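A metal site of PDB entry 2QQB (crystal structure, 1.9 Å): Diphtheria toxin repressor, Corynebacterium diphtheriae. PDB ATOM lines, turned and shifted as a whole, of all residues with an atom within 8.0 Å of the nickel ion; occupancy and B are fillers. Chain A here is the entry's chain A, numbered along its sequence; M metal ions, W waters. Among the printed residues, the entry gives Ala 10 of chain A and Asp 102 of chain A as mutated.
The guanidinium group (NE) of Arg 13 lies within salt-bridge range of the side-chain carboxylate (OE1) of Glu 105, at 3.0 Å. OD1 of Asp 102 lies close to NH2 of Arg 13 (2.8 Å). OE1 of Glu 105 lies close to ND1 of His 79. A ring nitrogen (ND1) of His 106 is in hydrogen-bond range of the side-chain carboxylate (OE1) of Glu 9, 2.8 Å away. NE2 of His 106 sits close to O of Leu 4.
A ring nitrogen (NE2) of His 106 binds the nickel ion (2.1 Å). Water W2 is bound to the nickel ion. The nickel ion is bound by O of Asp 102 (2.2 Å). The nickel ion is bound by OE2 of Glu 105 (2.3 Å). Water W1 is bound to the nickel ion, at 2.3 Å. The side-chain carboxylate (OD1) of Asp 102 binds the nickel ion.
Arg 13 touches the nickel ion.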
ATOM      1  N   ASP A   3     -30.200  12.084 -23.490  1.00  0.00           N
ATOM      2  CA  ASP A   3     -30.473  10.960 -24.465  1.00  0.00           C
ATOM      3  C   ASP A   3     -29.545  11.156 -25.676  1.00  0.00           C
ATOM      4  O   ASP A   3     -28.379  11.506 -25.451  1.00  0.00           O
ATOM      5  CB  ASP A   3     -31.964  10.901 -24.852  1.00  0.00           C
ATOM      6  CG  ASP A   3     -32.486   9.430 -25.093  1.00  0.00           C
ATOM      7  OD1 ASP A   3     -32.467   8.627 -24.121  1.00  0.00           O
ATOM      8  OD2 ASP A   3     -32.950   9.111 -26.243  1.00  0.00           O
ATOM      9  N   LEU A   4     -30.025  10.917 -26.903  1.00  0.00           N
ATOM     10  CA  LEU A   4     -29.252  11.155 -28.178  1.00  0.00           C
ATOM     11  C   LEU A   4     -28.995  12.635 -28.541  1.00  0.00           C
ATOM     12  O   LEU A   4     -28.247  12.892 -29.526  1.00  0.00           O
ATOM     13  CB  LEU A   4     -29.914  10.426 -29.393  1.00  0.00           C
ATOM     14  CG  LEU A   4     -29.470   9.041 -29.949  1.00  0.00           C
ATOM     15  CD1 LEU A   4     -29.616   7.907 -28.977  1.00  0.00           C
ATOM     16  CD2 LEU A   4     -30.279   8.685 -31.183  1.00  0.00           C
ATOM     17  N   VAL A   5     -29.615  13.559 -27.769  1.00  0.00           N
ATOM     18  CA  VAL A   5     -29.580  15.050 -27.942  1.00  0.00           C
ATOM     19  C   VAL A   5     -30.178  15.513 -29.290  1.00  0.00           C
ATOM     20  O   VAL A   5     -31.200  16.228 -29.334  1.00  0.00           O
ATOM     21  CB  VAL A   5     -28.146  15.690 -27.718  1.00  0.00           C
ATOM     22  CG1 VAL A   5     -28.176  17.191 -27.811  1.00  0.00           C
ATOM     23  CG2 VAL A   5     -27.506  15.237 -26.384  1.00  0.00           C
ATOM     24  N   ASP A   6     -29.498  15.147 -30.364  1.00  0.00           N
ATOM     25  CA  ASP A   6     -30.014  15.335 -31.728  1.00  0.00           C
ATOM     26  C   ASP A   6     -29.996  14.015 -32.557  1.00  0.00           C
ATOM     27  O   ASP A   6     -28.949  13.559 -32.934  1.00  0.00           O
ATOM     28  CB  ASP A   6     -29.269  16.462 -32.437  1.00  0.00           C
ATOM     29  CG  ASP A   6     -29.908  16.821 -33.770  1.00  0.00           C
ATOM     30  OD1 ASP A   6     -29.915  15.982 -34.702  1.00  0.00           O
ATOM     31  OD2 ASP A   6     -30.397  17.971 -33.884  1.00  0.00           O
ATOM     32  N   THR A   7     -31.164  13.485 -32.865  1.00  0.00           N
ATOM     33  CA  THR A   7     -31.343  12.109 -33.393  1.00  0.00           C
ATOM     34  C   THR A   7     -30.736  11.934 -34.795  1.00  0.00           C
ATOM     35  O   THR A   7     -29.948  11.003 -35.050  1.00  0.00           O
ATOM     36  CB  THR A   7     -32.841  11.688 -33.382  1.00  0.00           C
ATOM     37  OG1 THR A   7     -33.282  11.532 -32.022  1.00  0.00           O
ATOM     38  CG2 THR A   7     -33.047  10.368 -34.186  1.00  0.00           C
ATOM     39  N   GLU A   9     -28.595  13.904 -36.257  1.00  0.00           N
ATOM     40  CA  GLU A   9     -27.128  14.071 -36.181  1.00  0.00           C
ATOM     41  C   GLU A   9     -26.387  12.773 -35.645  1.00  0.00           C
ATOM     42  O   GLU A   9     -25.457  12.264 -36.290  1.00  0.00           O
ATOM     43  CB  GLU A   9     -26.814  15.333 -35.364  1.00  0.00           C
ATOM     44  CG  GLU A   9     -27.144  16.764 -36.049  1.00  0.00           C
ATOM     45  CD  GLU A   9     -26.644  17.929 -35.193  1.00  0.00           C
ATOM     46  OE1 GLU A   9     -26.262  17.676 -34.031  1.00  0.00           O
ATOM     47  OE2 GLU A   9     -26.540  19.074 -35.680  1.00  0.00           O
ATOM     48  N   ALA A  10     -26.837  12.193 -34.514  1.00  0.00           N
ATOM     49  CA  ALA A  10     -26.449  10.776 -34.153  1.00  0.00           C
ATOM     50  C   ALA A  10     -26.311   9.732 -35.318  1.00  0.00           C
ATOM     51  O   ALA A  10     -25.328   8.966 -35.374  1.00  0.00           O
ATOM     52  CB  ALA A  10     -27.382  10.191 -33.115  1.00  0.00           C
ATOM     53  N   TYR A  11     -27.365   9.633 -36.141  1.00  0.00           N
ATOM     54  CA  TYR A  11     -27.410   8.709 -37.281  1.00  0.00           C
ATOM     55  C   TYR A  11     -26.429   9.067 -38.359  1.00  0.00           C
ATOM     56  O   TYR A  11     -25.914   8.154 -39.045  1.00  0.00           O
ATOM     57  CB  TYR A  11     -28.817   8.712 -37.896  1.00  0.00           C
ATOM     58  CG  TYR A  11     -29.871   7.900 -37.109  1.00  0.00           C
ATOM     59  CD1 TYR A  11     -30.167   8.143 -35.739  1.00  0.00           C
ATOM     60  CD2 TYR A  11     -30.661   6.958 -37.774  1.00  0.00           C
ATOM     61  CE1 TYR A  11     -31.172   7.377 -35.067  1.00  0.00           C
ATOM     62  CE2 TYR A  11     -31.626   6.191 -37.108  1.00  0.00           C
ATOM     63  CZ  TYR A  11     -31.931   6.410 -35.765  1.00  0.00           C
ATOM     64  OH  TYR A  11     -32.953   5.556 -35.183  1.00  0.00           O
ATOM     65  N   ARG A  13     -23.483  10.965 -37.943  1.00  0.00           N
ATOM     66  CA  ARG A  13     -22.137  10.700 -37.395  1.00  0.00           C
ATOM     67  C   ARG A  13     -21.885   9.142 -37.326  1.00  0.00           C
ATOM     68  O   ARG A  13     -20.763   8.687 -37.564  1.00  0.00           O
ATOM     69  CB  ARG A  13     -22.001  11.384 -36.015  1.00  0.00           C
ATOM     70  CG  ARG A  13     -20.606  11.868 -35.633  1.00  0.00           C
ATOM     71  CD  ARG A  13     -19.850  10.936 -34.653  1.00  0.00           C
ATOM     72  NE  ARG A  13     -20.384  11.130 -33.269  1.00  0.00           N
ATOM     73  CZ  ARG A  13     -20.556  10.180 -32.374  1.00  0.00           C
ATOM     74  NH1 ARG A  13     -20.168   8.950 -32.659  1.00  0.00           N
ATOM     75  NH2 ARG A  13     -21.090  10.450 -31.163  1.00  0.00           N
ATOM     76  N   LEU A  34     -26.214   2.207 -32.207  1.00  0.00           N
ATOM     77  CA  LEU A  34     -26.915   3.251 -31.453  1.00  0.00           C
ATOM     78  C   LEU A  34     -27.698   2.682 -30.315  1.00  0.00           C
ATOM     79  O   LEU A  34     -28.276   3.413 -29.518  1.00  0.00           O
ATOM     80  CB  LEU A  34     -27.777   4.119 -32.359  1.00  0.00           C
ATOM     81  CG  LEU A  34     -27.085   5.201 -33.232  1.00  0.00           C
ATOM     82  CD1 LEU A  34     -28.175   6.004 -33.989  1.00  0.00           C
ATOM     83  CD2 LEU A  34     -26.128   6.136 -32.405  1.00  0.00           C
ATOM     84  N   VAL A  75     -20.867  17.619 -37.825  1.00  0.00           N
ATOM     85  CA  VAL A  75     -21.083  16.878 -36.548  1.00  0.00           C
ATOM     86  C   VAL A  75     -19.799  16.188 -36.056  1.00  0.00           C
ATOM     87  O   VAL A  75     -19.419  16.347 -34.884  1.00  0.00           O
ATOM     88  CB  VAL A  75     -22.217  15.775 -36.539  1.00  0.00           C
ATOM     89  CG1 VAL A  75     -22.427  15.331 -35.166  1.00  0.00           C
ATOM     90  CG2 VAL A  75     -23.566  16.220 -37.111  1.00  0.00           C
ATOM     91  N   HIS A  79     -17.441  16.883 -32.752  1.00  0.00           N
ATOM     92  CA  HIS A  79     -17.299  15.797 -31.822  1.00  0.00           C
ATOM     93  C   HIS A  79     -15.840  15.673 -31.478  1.00  0.00           C
ATOM     94  O   HIS A  79     -15.473  15.721 -30.339  1.00  0.00           O
ATOM     95  CB  HIS A  79     -17.859  14.491 -32.396  1.00  0.00           C
ATOM     96  CG  HIS A  79     -17.661  13.354 -31.496  1.00  0.00           C
ATOM     97  ND1 HIS A  79     -18.422  13.165 -30.381  1.00  0.00           N
ATOM     98  CD2 HIS A  79     -16.725  12.345 -31.506  1.00  0.00           C
ATOM     99  CE1 HIS A  79     -17.992  12.100 -29.737  1.00  0.00           C
ATOM    100  NE2 HIS A  79     -16.987  11.576 -30.415  1.00  0.00           N
ATOM    101  N   HIS A  98     -15.356  10.756 -24.461  1.00  0.00           N
ATOM    102  CA  HIS A  98     -16.239  10.416 -25.571  1.00  0.00           C
ATOM    103  C   HIS A  98     -17.709  10.699 -25.258  1.00  0.00           C
ATOM    104  O   HIS A  98     -18.435  11.263 -26.081  1.00  0.00           O
ATOM    105  CB  HIS A  98     -16.033   8.982 -26.191  1.00  0.00           C
ATOM    106  CG  HIS A  98     -17.210   8.546 -27.056  1.00  0.00           C
ATOM    107  ND1 HIS A  98     -17.411   8.999 -28.340  1.00  0.00           N
ATOM    108  CD2 HIS A  98     -18.304   7.830 -26.750  1.00  0.00           C
ATOM    109  CE1 HIS A  98     -18.531   8.492 -28.812  1.00  0.00           C
ATOM    110  NE2 HIS A  98     -19.147   7.889 -27.835  1.00  0.00           N
ATOM    111  N   ASP A  99     -18.174  10.204 -24.076  1.00  0.00           N
ATOM    112  CA  ASP A  99     -19.594  10.232 -23.782  1.00  0.00           C
ATOM    113  C   ASP A  99     -20.080  11.719 -23.686  1.00  0.00           C
ATOM    114  O   ASP A  99     -21.225  12.138 -24.052  1.00  0.00           O
ATOM    115  CB  ASP A  99     -19.821   9.466 -22.452  1.00  0.00           C
ATOM    116  CG  ASP A  99     -19.820   7.946 -22.648  1.00  0.00           C
ATOM    117  OD1 ASP A  99     -20.015   7.476 -23.800  1.00  0.00           O
ATOM    118  OD2 ASP A  99     -19.669   7.215 -21.624  1.00  0.00           O
ATOM    119  N   GLU A 100     -19.224  12.482 -23.100  1.00  0.00           N
ATOM    120  CA  GLU A 100     -19.418  13.912 -23.010  1.00  0.00           C
ATOM    121  C   GLU A 100     -19.479  14.583 -24.396  1.00  0.00           C
ATOM    122  O   GLU A 100     -20.459  15.229 -24.661  1.00  0.00           O
ATOM    123  CB  GLU A 100     -18.334  14.583 -22.185  1.00  0.00           C
ATOM    124  CG  GLU A 100     -18.684  16.019 -21.858  1.00  0.00           C
ATOM    125  CD  GLU A 100     -19.407  16.135 -20.495  1.00  0.00           C
ATOM    126  OE1 GLU A 100     -19.191  15.267 -19.580  1.00  0.00           O
ATOM    127  OE2 GLU A 100     -20.119  17.144 -20.339  1.00  0.00           O
ATOM    128  N   ALA A 101     -18.412  14.410 -25.187  1.00  0.00           N
ATOM    129  CA  ALA A 101     -18.339  14.886 -26.648  1.00  0.00           C
ATOM    130  C   ALA A 101     -19.573  14.415 -27.475  1.00  0.00           C
ATOM    131  O   ALA A 101     -19.967  15.084 -28.412  1.00  0.00           O
ATOM    132  CB  ALA A 101     -17.081  14.442 -27.327  1.00  0.00           C
ATOM    133  N   ASP A 102     -20.196  13.313 -27.041  1.00  0.00           N
ATOM    134  CA  ASP A 102     -21.426  12.766 -27.668  1.00  0.00           C
ATOM    135  C   ASP A 102     -22.626  13.758 -27.376  1.00  0.00           C
ATOM    136  O   ASP A 102     -23.616  13.811 -28.053  1.00  0.00           O
ATOM    137  CB  ASP A 102     -21.670  11.310 -27.093  1.00  0.00           C
ATOM    138  CG  ASP A 102     -22.603  10.412 -27.988  1.00  0.00           C
ATOM    139  OD1 ASP A 102     -22.991  10.821 -29.079  1.00  0.00           O
ATOM    140  OD2 ASP A 102     -22.929   9.232 -27.568  1.00  0.00           O
ATOM    141  N   ARG A 103     -22.536  14.542 -26.313  1.00  0.00           N
ATOM    142  CA  ARG A 103     -23.605  15.513 -26.075  1.00  0.00           C
ATOM    143  C   ARG A 103     -23.167  16.845 -26.720  1.00  0.00           C
ATOM    144  O   ARG A 103     -23.910  17.442 -27.469  1.00  0.00           O
ATOM    145  CB  ARG A 103     -23.951  15.651 -24.589  1.00  0.00           C
ATOM    146  CG  ARG A 103     -24.476  14.304 -23.894  1.00  0.00           C
ATOM    147  CD  ARG A 103     -24.975  14.548 -22.437  1.00  0.00           C
ATOM    148  NE  ARG A 103     -23.938  14.935 -21.551  1.00  0.00           N
ATOM    149  CZ  ARG A 103     -23.004  14.139 -20.978  1.00  0.00           C
ATOM    150  NH1 ARG A 103     -22.969  12.825 -21.160  1.00  0.00           N
ATOM    151  NH2 ARG A 103     -22.111  14.696 -20.201  1.00  0.00           N
ATOM    152  N   TRP A 104     -21.900  17.218 -26.504  1.00  0.00           N
ATOM    153  CA  TRP A 104     -21.421  18.501 -26.991  1.00  0.00           C
ATOM    154  C   TRP A 104     -21.382  18.609 -28.520  1.00  0.00           C
ATOM    155  O   TRP A 104     -21.540  19.697 -29.025  1.00  0.00           O
ATOM    156  CB  TRP A 104     -20.073  18.893 -26.407  1.00  0.00           C
ATOM    157  CG  TRP A 104     -20.039  19.054 -24.942  1.00  0.00           C
ATOM    158  CD1 TRP A 104     -20.845  18.449 -23.987  1.00  0.00           C
ATOM    159  CD2 TRP A 104     -19.040  19.792 -24.190  1.00  0.00           C
ATOM    160  NE1 TRP A 104     -20.437  18.831 -22.751  1.00  0.00           N
ATOM    161  CE2 TRP A 104     -19.340  19.616 -22.815  1.00  0.00           C
ATOM    162  CE3 TRP A 104     -17.934  20.590 -24.549  1.00  0.00           C
ATOM    163  CZ2 TRP A 104     -18.586  20.204 -21.811  1.00  0.00           C
ATOM    164  CZ3 TRP A 104     -17.184  21.178 -23.573  1.00  0.00           C
ATOM    165  CH2 TRP A 104     -17.497  20.943 -22.187  1.00  0.00           C
ATOM    166  N   GLU A 105     -21.161  17.491 -29.239  1.00  0.00           N
ATOM    167  CA  GLU A 105     -21.212  17.542 -30.719  1.00  0.00           C
ATOM    168  C   GLU A 105     -22.482  18.210 -31.334  1.00  0.00           C
ATOM    169  O   GLU A 105     -22.425  18.829 -32.429  1.00  0.00           O
ATOM    170  CB  GLU A 105     -21.097  16.174 -31.298  1.00  0.00           C
ATOM    171  CG  GLU A 105     -22.250  15.255 -31.059  1.00  0.00           C
ATOM    172  CD  GLU A 105     -21.779  13.937 -31.663  1.00  0.00           C
ATOM    173  OE1 GLU A 105     -20.908  13.992 -32.577  1.00  0.00           O
ATOM    174  OE2 GLU A 105     -22.166  12.930 -31.171  1.00  0.00           O
ATOM    175  N   HIS A 106     -23.615  18.064 -30.622  1.00  0.00           N
ATOM    176  CA  HIS A 106     -24.870  18.651 -31.081  1.00  0.00           C
ATOM    177  C   HIS A 106     -25.135  20.143 -30.754  1.00  0.00           C
ATOM    178  O   HIS A 106     -26.119  20.748 -31.267  1.00  0.00           O
ATOM    179  CB  HIS A 106     -26.032  17.788 -30.664  1.00  0.00           C
ATOM    180  CG  HIS A 106     -25.785  16.329 -30.839  1.00  0.00           C
ATOM    181  ND1 HIS A 106     -25.735  15.734 -32.076  1.00  0.00           N
ATOM    182  CD2 HIS A 106     -25.426  15.372 -29.951  1.00  0.00           C
ATOM    183  CE1 HIS A 106     -25.422  14.467 -31.948  1.00  0.00           C
ATOM    184  NE2 HIS A 106     -25.296  14.192 -30.656  1.00  0.00           N
HETATM  185 NI    NI M   1     -24.084  12.704 -29.907  1.00  0.00          NI
HETATM  186  O   HOH W   1     -24.681  11.072 -31.450  1.00  0.00           O
HETATM  187  O   HOH W   2     -25.747  11.908 -28.881  1.00  0.00           O
